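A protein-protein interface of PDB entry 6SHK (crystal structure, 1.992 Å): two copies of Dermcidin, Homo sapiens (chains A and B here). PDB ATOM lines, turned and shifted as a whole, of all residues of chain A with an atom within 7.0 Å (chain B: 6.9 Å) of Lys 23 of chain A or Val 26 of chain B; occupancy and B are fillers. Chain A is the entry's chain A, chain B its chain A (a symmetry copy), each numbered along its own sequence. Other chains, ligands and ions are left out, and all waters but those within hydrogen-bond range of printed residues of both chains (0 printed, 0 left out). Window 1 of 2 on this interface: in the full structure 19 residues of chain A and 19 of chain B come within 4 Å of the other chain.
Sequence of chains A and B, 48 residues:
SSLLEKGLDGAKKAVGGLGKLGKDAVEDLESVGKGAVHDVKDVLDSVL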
ATOM      1  N   GLY A  17      -7.810 -17.129   7.581  1.00  0.00           N
ATOM      2  CA  GLY A  17      -6.676 -16.372   7.083  1.00  0.00           C
ATOM      3  C   GLY A  17      -6.605 -14.968   7.656  1.00  0.00           C
ATOM      4  O   GLY A  17      -5.529 -14.489   8.027  1.00  0.00           O
ATOM      5  N   LEU A  18      -7.751 -14.290   7.745  1.00  0.00           N
ATOM      6  CA  LEU A  18      -7.757 -12.958   8.340  1.00  0.00           C
ATOM      7  C   LEU A  18      -7.369 -13.012   9.810  1.00  0.00           C
ATOM      8  O   LEU A  18      -6.597 -12.168  10.284  1.00  0.00           O
ATOM      9  CB  LEU A  18      -9.124 -12.305   8.181  1.00  0.00           C
ATOM     10  CG  LEU A  18      -9.529 -11.924   6.761  1.00  0.00           C
ATOM     11  CD1 LEU A  18     -10.822 -11.144   6.780  1.00  0.00           C
ATOM     12  CD2 LEU A  18      -8.430 -11.121   6.133  1.00  0.00           C
ATOM     13  N   GLY A  19      -7.908 -13.985  10.554  1.00  0.00           N
ATOM     14  CA  GLY A  19      -7.484 -14.184  11.930  1.00  0.00           C
ATOM     15  C   GLY A  19      -5.990 -14.407  12.053  1.00  0.00           C
ATOM     16  O   GLY A  19      -5.337 -13.807  12.918  1.00  0.00           O
ATOM     17  N   LYS A  20      -5.424 -15.241  11.177  1.00  0.00           N
ATOM     18  CA  LYS A  20      -3.969 -15.392  11.113  1.00  0.00           C
ATOM     19  C   LYS A  20      -3.279 -14.045  10.894  1.00  0.00           C
ATOM     20  O   LYS A  20      -2.464 -13.612  11.717  1.00  0.00           O
ATOM     21  CB  LYS A  20      -3.621 -16.381  10.001  1.00  0.00           C
ATOM     22  CG  LYS A  20      -2.147 -16.549   9.670  1.00  0.00           C
ATOM     23  CD  LYS A  20      -2.002 -17.574   8.539  1.00  0.00           C
ATOM     24  CE  LYS A  20      -0.613 -17.578   7.935  1.00  0.00           C
ATOM     25  NZ  LYS A  20      -0.571 -18.494   6.767  1.00  0.00           N
ATOM     26  N   LEU A  21      -3.589 -13.379   9.772  1.00  0.00           N
ATOM     27  CA  LEU A  21      -3.050 -12.049   9.472  1.00  0.00           C
ATOM     28  C   LEU A  21      -3.222 -11.079  10.643  1.00  0.00           C
ATOM     29  O   LEU A  21      -2.307 -10.315  10.980  1.00  0.00           O
ATOM     30  CB  LEU A  21      -3.730 -11.505   8.209  1.00  0.00           C
ATOM     31  CG  LEU A  21      -3.608 -10.026   7.825  1.00  0.00           C
ATOM     32  CD1 LEU A  21      -2.200  -9.686   7.348  1.00  0.00           C
ATOM     33  CD2 LEU A  21      -4.650  -9.629   6.776  1.00  0.00           C
ATOM     34  N   GLY A  22      -4.387 -11.103  11.284  1.00  0.00           N
ATOM     35  CA  GLY A  22      -4.618 -10.220  12.413  1.00  0.00           C
ATOM     36  C   GLY A  22      -3.721 -10.535  13.596  1.00  0.00           C
ATOM     37  O   GLY A  22      -3.097  -9.637  14.171  1.00  0.00           O
ATOM     38  N   LYS A  23      -3.659 -11.813  13.985  1.00  0.00           N
ATOM     39  CA  LYS A  23      -2.848 -12.215  15.123  1.00  0.00           C
ATOM     40  C   LYS A  23      -1.388 -11.865  14.898  1.00  0.00           C
ATOM     41  O   LYS A  23      -0.731 -11.361  15.815  1.00  0.00           O
ATOM     42  CB  LYS A  23      -3.019 -13.709  15.405  1.00  0.00           C
ATOM     43  CG  LYS A  23      -4.165 -14.019  16.385  1.00  0.00           C
ATOM     44  CD  LYS A  23      -4.772 -15.418  16.184  1.00  0.00           C
ATOM     45  CE  LYS A  23      -3.945 -16.522  16.842  1.00  0.00           C
ATOM     46  NZ  LYS A  23      -4.599 -17.864  16.763  1.00  0.00           N
ATOM     47  N   ASP A  24      -0.885 -12.077  13.673  1.00  0.00           N
ATOM     48  CA  ASP A  24       0.480 -11.678  13.324  1.00  0.00           C
ATOM     49  C   ASP A  24       0.697 -10.184  13.539  1.00  0.00           C
ATOM     50  O   ASP A  24       1.748  -9.770  14.044  1.00  0.00           O
ATOM     51  CB  ASP A  24       0.788 -12.043  11.871  1.00  0.00           C
ATOM     52  CG  ASP A  24       2.250 -11.817  11.503  1.00  0.00           C
ATOM     53  OD1 ASP A  24       3.036 -12.786  11.567  1.00  0.00           O
ATOM     54  OD2 ASP A  24       2.613 -10.673  11.159  1.00  0.00           O
ATOM     55  N   ALA A  25      -0.280  -9.360  13.146  1.00  0.00           N
ATOM     56  CA  ALA A  25      -0.155  -7.913  13.299  1.00  0.00           C
ATOM     57  C   ALA A  25      -0.074  -7.519  14.763  1.00  0.00           C
ATOM     58  O   ALA A  25       0.804  -6.746  15.162  1.00  0.00           O
ATOM     59  CB  ALA A  25      -1.330  -7.198  12.634  1.00  0.00           C
ATOM     60  N   VAL A  26      -1.000  -8.025  15.579  1.00  0.00           N
ATOM     61  CA  VAL A  26      -0.978  -7.702  16.998  1.00  0.00           C
ATOM     62  C   VAL A  26       0.357  -8.108  17.617  1.00  0.00           C
ATOM     63  O   VAL A  26       1.014  -7.301  18.286  1.00  0.00           O
ATOM     64  CB  VAL A  26      -2.156  -8.356  17.728  1.00  0.00           C
ATOM     65  CG1 VAL A  26      -1.941  -8.282  19.213  1.00  0.00           C
ATOM     66  CG2 VAL A  26      -3.465  -7.665  17.349  1.00  0.00           C
ATOM     67  N   GLU A  27       0.785  -9.361  17.402  1.00  0.00           N
ATOM     68  CA  GLU A  27       2.042  -9.797  18.009  1.00  0.00           C
ATOM     69  C   GLU A  27       3.209  -8.930  17.542  1.00  0.00           C
ATOM     70  O   GLU A  27       4.044  -8.520  18.357  1.00  0.00           O
ATOM     71  CB  GLU A  27       2.305 -11.276  17.732  1.00  0.00           C
ATOM     72  CG  GLU A  27       1.806 -12.187  18.871  1.00  0.00           C
ATOM     73  CD  GLU A  27       2.913 -12.998  19.551  1.00  0.00           C
ATOM     74  OE1 GLU A  27       3.765 -13.572  18.835  1.00  0.00           O
ATOM     75  OE2 GLU A  27       2.922 -13.069  20.805  1.00  0.00           O
ATOM     76  N   ASP A  28       3.261  -8.610  16.245  1.00  0.00           N
ATOM     77  CA  ASP A  28       4.256  -7.665  15.736  1.00  0.00           C
ATOM     78  C   ASP A  28       4.252  -6.352  16.526  1.00  0.00           C
ATOM     79  O   ASP A  28       5.299  -5.890  16.988  1.00  0.00           O
ATOM     80  CB  ASP A  28       4.011  -7.401  14.246  1.00  0.00           C
ATOM     81  CG  ASP A  28       4.541  -8.511  13.355  1.00  0.00           C
ATOM     82  OD1 ASP A  28       5.088  -9.509  13.884  1.00  0.00           O
ATOM     83  OD2 ASP A  28       4.413  -8.380  12.118  1.00  0.00           O
ATOM     84  N   LEU A  29       3.073  -5.740  16.709  1.00  0.00           N
ATOM     85  CA  LEU A  29       3.036  -4.480  17.442  1.00  0.00           C
ATOM     86  C   LEU A  29       3.486  -4.664  18.891  1.00  0.00           C
ATOM     87  O   LEU A  29       4.241  -3.832  19.417  1.00  0.00           O
ATOM     88  CB  LEU A  29       1.642  -3.862  17.409  1.00  0.00           C
ATOM     89  CG  LEU A  29       0.969  -3.430  16.083  1.00  0.00           C
ATOM     90  CD1 LEU A  29      -0.534  -3.129  16.280  1.00  0.00           C
ATOM     91  CD2 LEU A  29       1.655  -2.233  15.427  1.00  0.00           C
ATOM     92  N   LEU B  21      -5.413  -7.216  25.034  1.00  0.00           N
ATOM     93  CA  LEU B  21      -6.682  -6.709  24.506  1.00  0.00           C
ATOM     94  C   LEU B  21      -6.809  -6.930  22.997  1.00  0.00           C
ATOM     95  O   LEU B  21      -7.869  -7.331  22.496  1.00  0.00           O
ATOM     96  CB  LEU B  21      -6.811  -5.220  24.851  1.00  0.00           C
ATOM     97  CG  LEU B  21      -7.871  -4.344  24.172  1.00  0.00           C
ATOM     98  CD1 LEU B  21      -9.276  -4.691  24.652  1.00  0.00           C
ATOM     99  CD2 LEU B  21      -7.579  -2.854  24.370  1.00  0.00           C
ATOM    100  N   GLY B  22      -5.731  -6.685  22.256  1.00  0.00           N
ATOM    101  CA  GLY B  22      -5.773  -6.885  20.819  1.00  0.00           C
ATOM    102  C   GLY B  22      -5.965  -8.341  20.435  1.00  0.00           C
ATOM    103  O   GLY B  22      -6.817  -8.666  19.601  1.00  0.00           O
ATOM    104  N   LYS B  23      -5.163  -9.233  21.026  1.00  0.00           N
ATOM    105  CA  LYS B  23      -5.250 -10.650  20.708  1.00  0.00           C
ATOM    106  C   LYS B  23      -6.634 -11.190  21.019  1.00  0.00           C
ATOM    107  O   LYS B  23      -7.192 -11.946  20.215  1.00  0.00           O
ATOM    108  CB  LYS B  23      -4.172 -11.438  21.456  1.00  0.00           C
ATOM    109  CG  LYS B  23      -2.853 -11.562  20.673  1.00  0.00           C
ATOM    110  CD  LYS B  23      -1.623 -11.729  21.580  1.00  0.00           C
ATOM    111  CE  LYS B  23      -1.439 -13.165  22.069  1.00  0.00           C
ATOM    112  NZ  LYS B  23      -0.173 -13.360  22.841  1.00  0.00           N
ATOM    113  N   ASP B  24      -7.220 -10.771  22.151  1.00  0.00           N
ATOM    114  CA  ASP B  24      -8.593 -11.150  22.491  1.00  0.00           C
ATOM    115  C   ASP B  24      -9.576 -10.721  21.408  1.00  0.00           C
ATOM    116  O   ASP B  24     -10.491 -11.475  21.057  1.00  0.00           O
ATOM    117  CB  ASP B  24      -9.000 -10.539  23.832  1.00  0.00           C
ATOM    118  CG  ASP B  24     -10.350 -11.043  24.326  1.00  0.00           C
ATOM    119  OD1 ASP B  24     -10.371 -11.998  25.131  1.00  0.00           O
ATOM    120  OD2 ASP B  24     -11.388 -10.491  23.905  1.00  0.00           O
ATOM    121  N   ALA B  25      -9.411  -9.503  20.879  1.00  0.00           N
ATOM    122  CA  ALA B  25     -10.311  -9.000  19.846  1.00  0.00           C
ATOM    123  C   ALA B  25     -10.218  -9.833  18.580  1.00  0.00           C
ATOM    124  O   ALA B  25     -11.238 -10.248  18.019  1.00  0.00           O
ATOM    125  CB  ALA B  25     -10.003  -7.537  19.528  1.00  0.00           C
ATOM    126  N   VAL B  26      -8.997 -10.069  18.099  1.00  0.00           N
ATOM    127  CA  VAL B  26      -8.828 -10.871  16.897  1.00  0.00           C
ATOM    128  C   VAL B  26      -9.452 -12.252  17.084  1.00  0.00           C
ATOM    129  O   VAL B  26     -10.251 -12.701  16.253  1.00  0.00           O
ATOM    130  CB  VAL B  26      -7.349 -10.973  16.507  1.00  0.00           C
ATOM    131  CG1 VAL B  26      -7.166 -12.048  15.474  1.00  0.00           C
ATOM    132  CG2 VAL B  26      -6.849  -9.634  15.969  1.00  0.00           C
ATOM    133  N   GLU B  27      -9.106 -12.946  18.178  1.00  0.00           N
ATOM    134  CA  GLU B  27      -9.656 -14.287  18.373  1.00  0.00           C
ATOM    135  C   GLU B  27     -11.181 -14.254  18.433  1.00  0.00           C
ATOM    136  O   GLU B  27     -11.846 -15.089  17.810  1.00  0.00           O
ATOM    137  CB  GLU B  27      -9.066 -14.950  19.616  1.00  0.00           C
ATOM    138  CG  GLU B  27      -7.851 -15.840  19.291  1.00  0.00           C
ATOM    139  CD  GLU B  27      -8.047 -17.318  19.643  1.00  0.00           C
ATOM    140  OE1 GLU B  27      -8.554 -17.609  20.750  1.00  0.00           O
ATOM    141  OE2 GLU B  27      -7.682 -18.187  18.813  1.00  0.00           O
ATOM    142  N   ASP B  28     -11.750 -13.274  19.143  1.00  0.00           N
ATOM    143  CA  ASP B  28     -13.200 -13.076  19.137  1.00  0.00           C
ATOM    144  C   ASP B  28     -13.755 -12.982  17.711  1.00  0.00           C
ATOM    145  O   ASP B  28     -14.707 -13.683  17.358  1.00  0.00           O
ATOM    146  CB  ASP B  28     -13.559 -11.822  19.942  1.00  0.00           C
ATOM    147  CG  ASP B  28     -13.553 -12.061  21.442  1.00  0.00           C
ATOM    148  OD1 ASP B  28     -13.249 -13.199  21.876  1.00  0.00           O
ATOM    149  OD2 ASP B  28     -13.856 -11.105  22.188  1.00  0.00           O
ATOM    150  N   LEU B  29     -13.160 -12.128  16.867  1.00  0.00           N
ATOM    151  CA  LEU B  29     -13.675 -12.001  15.509  1.00  0.00           C
ATOM    152  C   LEU B  29     -13.531 -13.310  14.733  1.00  0.00           C
ATOM    153  O   LEU B  29     -14.458 -13.711  14.012  1.00  0.00           O
ATOM    154  CB  LEU B  29     -12.974 -10.876  14.755  1.00  0.00           C
ATOM    155  CG  LEU B  29     -13.060  -9.401  15.221  1.00  0.00           C
ATOM    156  CD1 LEU B  29     -12.030  -8.512  14.486  1.00  0.00           C
ATOM    157  CD2 LEU B  29     -14.459  -8.807  15.067  1.00  0.00           C
ATOM    158  N   GLU B  30     -12.359 -13.955  14.826  1.00  0.00           N
ATOM    159  CA  GLU B  30     -12.170 -15.276  14.221  1.00  0.00           C
ATOM    160  C   GLU B  30     -13.358 -16.176  14.549  1.00  0.00           C
ATOM    161  O   GLU B  30     -14.051 -16.674  13.653  1.00  0.00           O
ATOM    162  CB  GLU B  30     -10.849 -15.904  14.705  1.00  0.00           C
ATOM    163  CG  GLU B  30     -10.313 -17.123  13.904  1.00  0.00           C
ATOM    164  CD  GLU B  30      -8.888 -17.575  14.323  1.00  0.00           C
ATOM    165  OE1 GLU B  30      -8.391 -17.131  15.382  1.00  0.00           O
ATOM    166  OE2 GLU B  30      -8.259 -18.379  13.592  1.00  0.00           O
ATOM    167  N   SER B  31     -13.649 -16.336  15.843  1.00  0.00           N
ATOM    168  CA  SER B  31     -14.715 -17.243  16.236  1.00  0.00           C
ATOM    169  C   SER B  31     -16.076 -16.726  15.772  1.00  0.00           C
ATOM    170  O   SER B  31     -16.916 -17.517  15.334  1.00  0.00           O
ATOM    171  CB  SER B  31     -14.672 -17.470  17.751  1.00  0.00           C
ATOM    172  OG  SER B  31     -15.579 -16.635  18.437  1.00  0.00           O
ATOM    173  N   VAL B  32     -16.281 -15.407  15.801  1.00  0.00           N
ATOM    174  CA  VAL B  32     -17.537 -14.833  15.317  1.00  0.00           C
ATOM    175  C   VAL B  32     -17.756 -15.192  13.852  1.00  0.00           C
ATOM    176  O   VAL B  32     -18.854 -15.591  13.448  1.00  0.00           O
ATOM    177  CB  VAL B  32     -17.543 -13.311  15.530  1.00  0.00           C
ATOM    178  CG1 VAL B  32     -18.529 -12.628  14.594  1.00  0.00           C
ATOM    179  CG2 VAL B  32     -17.869 -12.995  16.977  1.00  0.00           C
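Hydrophobic or aromatic side chains of chain A within 4 Å of the printed part of chain B: Val 26.
Lys 23 of chain A touches two residues of chain B. Of chain A, only Gly 19 and Lys 23 come within 4 Å of Val 26 of chain B. Of the printed residues of chain B, Gly 19 of chain A touches Val 26 (3.6 Å). Printed residues of chain B within 4 Å of Val 26 of chain A: Lys 23. Printed residues of chain A within 4 Å of Glu 27 of chain B: Lys 23. Of the printed residues of chain B, Glu 27 of chain A touches Lys 23. The nearest residue of chain A that does not touch Val 26 of chain B is Gly 22 of chain A (4.03 Å). The nearest printed residue of chain B that does not touch Glu 27 of chain A is Gly 22 of chain B (7.5 Å).
The side-chain amino group (NZ) of Lys 23 of chain B is in salt-bridge range of the side-chain carboxylate (OE2) of Glu 27 of chain A (3.7 Å). NZ of Lys 23 of chain A is in salt-bridge range of OE2 of Glu 27 of chain B (3.7 Å).
Among the printed residues, merely in contact across the chains: Gly 19 of chain A with Val 26 of chain B (3.6 Å), Lys 23 of chain A with Val 26 of chain B (3.7 Å) and Val 26 of chain A with Lys 23 of chain B (3.7 Å).
Lys 23 of chain A touches Val 26 of chain B, and with the chains exchanged Val 26 of chain A touches Lys 23 of chain B. Lys 23 of chain A touches Glu 27 of chain B, and with the chains exchanged Glu 27 of chain A touches Lys 23 of chain B. Positions printed for both chains: 21, 22, 23, 24, 25, 26, 27, 28 and 29.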
